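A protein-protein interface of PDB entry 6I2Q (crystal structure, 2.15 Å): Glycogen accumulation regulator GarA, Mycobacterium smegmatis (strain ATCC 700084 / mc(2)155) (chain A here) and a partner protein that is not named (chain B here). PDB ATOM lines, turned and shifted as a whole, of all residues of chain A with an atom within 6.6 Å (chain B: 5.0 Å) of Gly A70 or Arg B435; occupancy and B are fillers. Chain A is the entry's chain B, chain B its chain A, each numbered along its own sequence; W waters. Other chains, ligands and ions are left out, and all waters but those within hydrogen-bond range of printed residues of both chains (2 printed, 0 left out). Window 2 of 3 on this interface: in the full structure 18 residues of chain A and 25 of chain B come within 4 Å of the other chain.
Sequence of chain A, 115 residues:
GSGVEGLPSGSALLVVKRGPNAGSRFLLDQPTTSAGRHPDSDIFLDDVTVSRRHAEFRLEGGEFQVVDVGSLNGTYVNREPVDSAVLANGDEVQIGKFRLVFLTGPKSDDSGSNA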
ATOM      1  N   SER A  51     -11.237  -3.184 -22.485  1.00  0.00           N
ATOM      2  CA  SER A  51     -10.068  -3.646 -21.757  1.00  0.00           C
ATOM      3  C   SER A  51     -10.498  -4.647 -20.687  1.00  0.00           C
ATOM      4  O   SER A  51     -11.638  -4.577 -20.199  1.00  0.00           O
ATOM      5  CB  SER A  51      -9.306  -2.468 -21.158  1.00  0.00           C
ATOM      6  OG  SER A  51      -8.845  -1.594 -22.179  1.00  0.00           O
ATOM      7  N   ARG A  52      -9.582  -5.594 -20.344  1.00  0.00           N
ATOM      8  CA  ARG A  52      -9.741  -6.639 -19.317  1.00  0.00           C
ATOM      9  C   ARG A  52     -10.420  -6.036 -18.064  1.00  0.00           C
ATOM     10  O   ARG A  52     -11.429  -6.570 -17.587  1.00  0.00           O
ATOM     11  CB  ARG A  52      -8.365  -7.270 -18.991  1.00  0.00           C
ATOM     12  CG  ARG A  52      -8.381  -8.338 -17.883  1.00  0.00           C
ATOM     13  CD  ARG A  52      -7.005  -8.954 -17.714  1.00  0.00           C
ATOM     14  NE  ARG A  52      -6.901  -9.808 -16.528  1.00  0.00           N
ATOM     15  CZ  ARG A  52      -6.606  -9.362 -15.308  1.00  0.00           C
ATOM     16  NH1 ARG A  52      -6.405  -8.065 -15.097  1.00  0.00           N
ATOM     17  NH2 ARG A  52      -6.520 -10.208 -14.289  1.00  0.00           N
ATOM     18  N   ARG A  53      -9.885  -4.909 -17.572  1.00  0.00           N
ATOM     19  CA  ARG A  53     -10.463  -4.099 -16.496  1.00  0.00           C
ATOM     20  C   ARG A  53     -10.709  -2.757 -17.157  1.00  0.00           C
ATOM     21  O   ARG A  53      -9.757  -2.159 -17.679  1.00  0.00           O
ATOM     22  CB  ARG A  53      -9.560  -4.040 -15.249  1.00  0.00           C
ATOM     23  CG  ARG A  53      -9.230  -5.403 -14.616  1.00  0.00           C
ATOM     24  CD  ARG A  53     -10.445  -6.198 -14.159  1.00  0.00           C
ATOM     25  NE  ARG A  53     -10.069  -7.442 -13.483  1.00  0.00           N
ATOM     26  CZ  ARG A  53     -10.922  -8.252 -12.864  1.00  0.00           C
ATOM     27  NH1 ARG A  53     -12.218  -7.963 -12.827  1.00  0.00           N
ATOM     28  NH2 ARG A  53     -10.487  -9.354 -12.270  1.00  0.00           N
ATOM     29  N   HIS A  54     -11.992  -2.367 -17.310  1.00  0.00           N
ATOM     30  CA  HIS A  54     -12.341  -1.191 -18.114  1.00  0.00           C
ATOM     31  C   HIS A  54     -13.090  -0.125 -17.312  1.00  0.00           C
ATOM     32  O   HIS A  54     -12.628   1.018 -17.227  1.00  0.00           O
ATOM     33  CB  HIS A  54     -13.183  -1.633 -19.337  1.00  0.00           C
ATOM     34  CG  HIS A  54     -13.279  -0.617 -20.435  1.00  0.00           C
ATOM     35  ND1 HIS A  54     -12.732  -0.857 -21.685  1.00  0.00           N
ATOM     36  CD2 HIS A  54     -13.847   0.613 -20.439  1.00  0.00           C
ATOM     37  CE1 HIS A  54     -12.993   0.220 -22.407  1.00  0.00           C
ATOM     38  NE2 HIS A  54     -13.653   1.135 -21.696  1.00  0.00           N
ATOM     39  N   ALA A  55     -14.257  -0.475 -16.770  1.00  0.00           N
ATOM     40  CA  ALA A  55     -15.060   0.484 -16.025  1.00  0.00           C
ATOM     41  C   ALA A  55     -15.661  -0.136 -14.770  1.00  0.00           C
ATOM     42  O   ALA A  55     -15.565  -1.348 -14.560  1.00  0.00           O
ATOM     43  CB  ALA A  55     -16.164   1.045 -16.917  1.00  0.00           C
ATOM     44  N   VAL A  67     -17.150   5.015 -13.595  1.00  0.00           N
ATOM     45  CA  VAL A  67     -15.747   5.351 -13.371  1.00  0.00           C
ATOM     46  C   VAL A  67     -14.883   4.484 -14.289  1.00  0.00           C
ATOM     47  O   VAL A  67     -15.023   3.260 -14.264  1.00  0.00           O
ATOM     48  CB  VAL A  67     -15.336   5.160 -11.866  1.00  0.00           C
ATOM     49  CG1 VAL A  67     -13.905   5.623 -11.613  1.00  0.00           C
ATOM     50  CG2 VAL A  67     -16.295   5.863 -10.907  1.00  0.00           C
ATOM     51  N   ASP A  68     -13.977   5.110 -15.065  1.00  0.00           N
ATOM     52  CA  ASP A  68     -13.025   4.385 -15.911  1.00  0.00           C
ATOM     53  C   ASP A  68     -11.858   3.952 -15.008  1.00  0.00           C
ATOM     54  O   ASP A  68     -11.349   4.767 -14.233  1.00  0.00           O
ATOM     55  CB  ASP A  68     -12.555   5.236 -17.116  1.00  0.00           C
ATOM     56  CG  ASP A  68     -11.735   4.433 -18.109  1.00  0.00           C
ATOM     57  OD1 ASP A  68     -12.260   4.126 -19.204  1.00  0.00           O
ATOM     58  OD2 ASP A  68     -10.573   4.093 -17.786  1.00  0.00           O
ATOM     59  N   VAL A  69     -11.469   2.663 -15.068  1.00  0.00           N
ATOM     60  CA  VAL A  69     -10.436   2.128 -14.167  1.00  0.00           C
ATOM     61  C   VAL A  69      -9.093   1.830 -14.899  1.00  0.00           C
ATOM     62  O   VAL A  69      -8.316   0.985 -14.448  1.00  0.00           O
ATOM     63  CB  VAL A  69     -10.928   0.898 -13.340  1.00  0.00           C
ATOM     64  CG1 VAL A  69     -11.949   1.311 -12.279  1.00  0.00           C
ATOM     65  CG2 VAL A  69     -11.470  -0.230 -14.220  1.00  0.00           C
ATOM     66  N   GLY A  70      -8.798   2.591 -15.947  1.00  0.00           N
ATOM     67  CA  GLY A  70      -7.531   2.474 -16.662  1.00  0.00           C
ATOM     68  C   GLY A  70      -7.595   1.738 -17.982  1.00  0.00           C
ATOM     69  O   GLY A  70      -6.625   1.079 -18.378  1.00  0.00           O
ATOM     70  N   SER A  71      -8.735   1.854 -18.670  1.00  0.00           N
ATOM     71  CA  SER A  71      -8.935   1.247 -19.983  1.00  0.00           C
ATOM     72  C   SER A  71      -8.148   1.995 -21.051  1.00  0.00           C
ATOM     73  O   SER A  71      -7.794   3.158 -20.854  1.00  0.00           O
ATOM     74  CB  SER A  71     -10.413   1.250 -20.341  1.00  0.00           C
ATOM     75  OG  SER A  71     -10.853   2.491 -20.868  1.00  0.00           O
ATOM     76  N   LEU A  72      -7.895   1.338 -22.183  1.00  0.00           N
ATOM     77  CA  LEU A  72      -7.195   1.959 -23.293  1.00  0.00           C
ATOM     78  C   LEU A  72      -8.122   2.885 -24.091  1.00  0.00           C
ATOM     79  O   LEU A  72      -7.692   3.982 -24.452  1.00  0.00           O
ATOM     80  CB  LEU A  72      -6.585   0.881 -24.219  1.00  0.00           C
ATOM     81  CG  LEU A  72      -5.789   1.309 -25.463  1.00  0.00           C
ATOM     82  CD1 LEU A  72      -4.739   2.407 -25.158  1.00  0.00           C
ATOM     83  CD2 LEU A  72      -5.100   0.120 -26.063  1.00  0.00           C
ATOM     84  N   LYS B 428       1.327   6.886 -17.989  1.00  0.00           N
ATOM     85  CA  LYS B 428       0.192   6.186 -17.386  1.00  0.00           C
ATOM     86  C   LYS B 428      -0.681   5.576 -18.477  1.00  0.00           C
ATOM     87  O   LYS B 428      -1.068   4.408 -18.375  1.00  0.00           O
ATOM     88  CB  LYS B 428      -0.636   7.141 -16.488  1.00  0.00           C
ATOM     89  CG  LYS B 428      -1.878   6.498 -15.859  1.00  0.00           C
ATOM     90  CD  LYS B 428      -2.758   7.519 -15.155  1.00  0.00           C
ATOM     91  CE  LYS B 428      -3.515   6.909 -13.994  1.00  0.00           C
ATOM     92  NZ  LYS B 428      -4.038   7.947 -13.060  1.00  0.00           N
ATOM     93  N   GLU B 431       1.072   2.737 -19.954  1.00  0.00           N
ATOM     94  CA  GLU B 431       0.949   1.620 -19.013  1.00  0.00           C
ATOM     95  C   GLU B 431      -0.411   0.952 -19.204  1.00  0.00           C
ATOM     96  O   GLU B 431      -0.466  -0.276 -19.284  1.00  0.00           O
ATOM     97  CB  GLU B 431       1.148   2.082 -17.569  1.00  0.00           C
ATOM     98  CG  GLU B 431       2.610   2.201 -17.178  1.00  0.00           C
ATOM     99  CD  GLU B 431       2.887   2.781 -15.802  1.00  0.00           C
ATOM    100  OE1 GLU B 431       1.991   2.730 -14.926  1.00  0.00           O
ATOM    101  OE2 GLU B 431       4.017   3.282 -15.601  1.00  0.00           O
ATOM    102  N   ASP B 432      -1.493   1.764 -19.359  1.00  0.00           N
ATOM    103  CA  ASP B 432      -2.853   1.289 -19.666  1.00  0.00           C
ATOM    104  C   ASP B 432      -2.853   0.437 -20.942  1.00  0.00           C
ATOM    105  O   ASP B 432      -3.521  -0.593 -20.981  1.00  0.00           O
ATOM    106  CB  ASP B 432      -3.849   2.466 -19.851  1.00  0.00           C
ATOM    107  CG  ASP B 432      -4.020   3.400 -18.670  1.00  0.00           C
ATOM    108  OD1 ASP B 432      -3.689   2.992 -17.534  1.00  0.00           O
ATOM    109  OD2 ASP B 432      -4.494   4.541 -18.882  1.00  0.00           O
ATOM    110  N   ALA B 433      -2.086   0.859 -21.963  1.00  0.00           N
ATOM    111  CA  ALA B 433      -1.981   0.155 -23.245  1.00  0.00           C
ATOM    112  C   ALA B 433      -1.257  -1.198 -23.082  1.00  0.00           C
ATOM    113  O   ALA B 433      -1.740  -2.204 -23.613  1.00  0.00           O
ATOM    114  CB  ALA B 433      -1.276   1.022 -24.272  1.00  0.00           C
ATOM    115  N   LEU B 434      -0.132  -1.229 -22.319  1.00  0.00           N
ATOM    116  CA  LEU B 434       0.615  -2.462 -22.031  1.00  0.00           C
ATOM    117  C   LEU B 434      -0.280  -3.431 -21.213  1.00  0.00           C
ATOM    118  O   LEU B 434      -0.252  -4.642 -21.456  1.00  0.00           O
ATOM    119  CB  LEU B 434       1.948  -2.160 -21.278  1.00  0.00           C
ATOM    120  CG  LEU B 434       2.854  -3.376 -20.903  1.00  0.00           C
ATOM    121  CD1 LEU B 434       3.263  -4.198 -22.141  1.00  0.00           C
ATOM    122  CD2 LEU B 434       4.095  -2.935 -20.189  1.00  0.00           C
ATOM    123  N   ARG B 435      -1.081  -2.880 -20.270  1.00  0.00           N
ATOM    124  CA  ARG B 435      -2.022  -3.637 -19.434  1.00  0.00           C
ATOM    125  C   ARG B 435      -3.076  -4.296 -20.333  1.00  0.00           C
ATOM    126  O   ARG B 435      -3.278  -5.512 -20.268  1.00  0.00           O
ATOM    127  CB  ARG B 435      -2.679  -2.701 -18.413  1.00  0.00           C
ATOM    128  CG  ARG B 435      -2.933  -3.346 -17.070  1.00  0.00           C
ATOM    129  CD  ARG B 435      -3.605  -2.410 -16.070  1.00  0.00           C
ATOM    130  NE  ARG B 435      -2.805  -1.209 -15.833  1.00  0.00           N
ATOM    131  CZ  ARG B 435      -3.218   0.027 -16.089  1.00  0.00           C
ATOM    132  NH1 ARG B 435      -4.440   0.240 -16.568  1.00  0.00           N
ATOM    133  NH2 ARG B 435      -2.417   1.062 -15.858  1.00  0.00           N
ATOM    134  N   ASP B 436      -3.672  -3.493 -21.238  1.00  0.00           N
ATOM    135  CA  ASP B 436      -4.663  -3.925 -22.223  1.00  0.00           C
ATOM    136  C   ASP B 436      -4.088  -5.063 -23.078  1.00  0.00           C
ATOM    137  O   ASP B 436      -4.769  -6.076 -23.265  1.00  0.00           O
ATOM    138  CB  ASP B 436      -5.101  -2.737 -23.097  1.00  0.00           C
ATOM    139  CG  ASP B 436      -6.036  -3.123 -24.232  1.00  0.00           C
ATOM    140  OD1 ASP B 436      -5.541  -3.598 -25.270  1.00  0.00           O
ATOM    141  OD2 ASP B 436      -7.261  -2.964 -24.071  1.00  0.00           O
ATOM    142  N   TYR B 437      -2.827  -4.913 -23.547  1.00  0.00           N
ATOM    143  CA  TYR B 437      -2.136  -5.901 -24.372  1.00  0.00           C
ATOM    144  C   TYR B 437      -2.021  -7.265 -23.654  1.00  0.00           C
ATOM    145  O   TYR B 437      -2.432  -8.285 -24.217  1.00  0.00           O
ATOM    146  CB  TYR B 437      -0.746  -5.395 -24.814  1.00  0.00           C
ATOM    147  CG  TYR B 437       0.067  -6.461 -25.522  1.00  0.00           C
ATOM    148  CD1 TYR B 437      -0.314  -6.939 -26.773  1.00  0.00           C
ATOM    149  CD2 TYR B 437       1.156  -7.067 -24.897  1.00  0.00           C
ATOM    150  CE1 TYR B 437       0.398  -7.950 -27.411  1.00  0.00           C
ATOM    151  CE2 TYR B 437       1.872  -8.085 -25.525  1.00  0.00           C
ATOM    152  CZ  TYR B 437       1.496  -8.513 -26.790  1.00  0.00           C
ATOM    153  OH  TYR B 437       2.181  -9.517 -27.433  1.00  0.00           O
ATOM    154  N   GLN B 438      -1.470  -7.270 -22.419  1.00  0.00           N
ATOM    155  CA  GLN B 438      -1.287  -8.466 -21.601  1.00  0.00           C
ATOM    156  C   GLN B 438      -2.655  -9.144 -21.328  1.00  0.00           C
ATOM    157  O   GLN B 438      -2.753 -10.373 -21.401  1.00  0.00           O
ATOM    158  CB  GLN B 438      -0.530  -8.123 -20.295  1.00  0.00           C
ATOM    159  CG  GLN B 438       0.943  -7.746 -20.545  1.00  0.00           C
ATOM    160  CD  GLN B 438       1.636  -7.043 -19.389  1.00  0.00           C
ATOM    161  OE1 GLN B 438       1.015  -6.407 -18.523  1.00  0.00           O
ATOM    162  NE2 GLN B 438       2.958  -7.120 -19.361  1.00  0.00           N
ATOM    163  N   GLY B 439      -3.694  -8.336 -21.106  1.00  0.00           N
ATOM    164  CA  GLY B 439      -5.056  -8.828 -20.920  1.00  0.00           C
ATOM    165  C   GLY B 439      -5.588  -9.536 -22.166  1.00  0.00           C
ATOM    166  O   GLY B 439      -6.268 -10.557 -22.046  1.00  0.00           O
HETATM  167  O   HOH W   1      -7.372  -6.127 -22.438  1.00  0.00           O
HETATM  168  O   HOH W   2      -5.862  -1.544 -19.920  1.00  0.00           O
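Water W1 lies within hydrogen-bond range of O of Asp B436 and N of Arg A52.
Water W2 lies within hydrogen-bond range of the backbone carbonyl oxygen of Asp B432 (2.7 Å), the backbone carbonyl oxygen of Gly A70 (3.1 Å) and the backbone NH of Asp B436 (3.2 Å).
Of the printed residues of chain B, Ser A51 touches Asp B436 (2.8 Å).
Of the printed residues of chain B, Arg A52 touches Gly B439.
His A54 touches none of the printed residues of chain B.
Of chain B, only Asp B432 and Arg B435 come within 4 Å of Gly A70.
Of the printed residues of chain B, Leu A72 touches Ala B433 (3.8 Å) and Asp B436 (3.8 Å).
Of the printed residues of chain A, Arg B435 touches Gly A70.
Printed residues of chain A within 4 Å of Asp B436: Ser A51 and Leu A72.
Printed residues of chain A within 4 Å of Gly B439: Arg A52 (3.8 Å).
The nearest printed residue of chain B that does not touch Ser A51 is Asp B432 (5.5 Å).
Gly B439 touches Arg A52.
O of Gly A70 touches CB of Asp B432, at 3.4 Å.
Leu A72 touches Ala B433.
Leu A72 touches Asp B436.
A ring nitrogen (ND1) of His A54 is in hydrogen-bond range of the backbone NH of Ser A51 (2.9 Å).
The side-chain carboxylate of Asp A68 lies within hydrogen-bond range of the backbone NH of Gly A70, 3.0 Å away.
The guanidinium group (NH2) of Arg B435 lies within salt-bridge range of the side-chain carboxylate (OD1) of Asp B432 (2.9 Å).
The side-chain hydroxyl (OG) of Ser A51 sits at hydrogen-bond distance from the backbone NH (N) of Leu A72, 3.1 Å away.
Hydrophobic or aromatic side chains of chain A within 4 Å of the printed part of chain B: Leu A72.
Of the 10 printed residues of chain B, 5 touch a printed residue of chain A.
Hydrophobic or aromatic side chains of chain B that line the printed part of chain A: Ala B433.
The backbone carbonyl oxygen (O) of Gly A70 lies within hydrogen-bond range of the guanidinium group (NH1) of Arg B435.
OG of Ser A51 is in hydrogen-bond range of OD2 of Asp B436 (2.8 Å).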
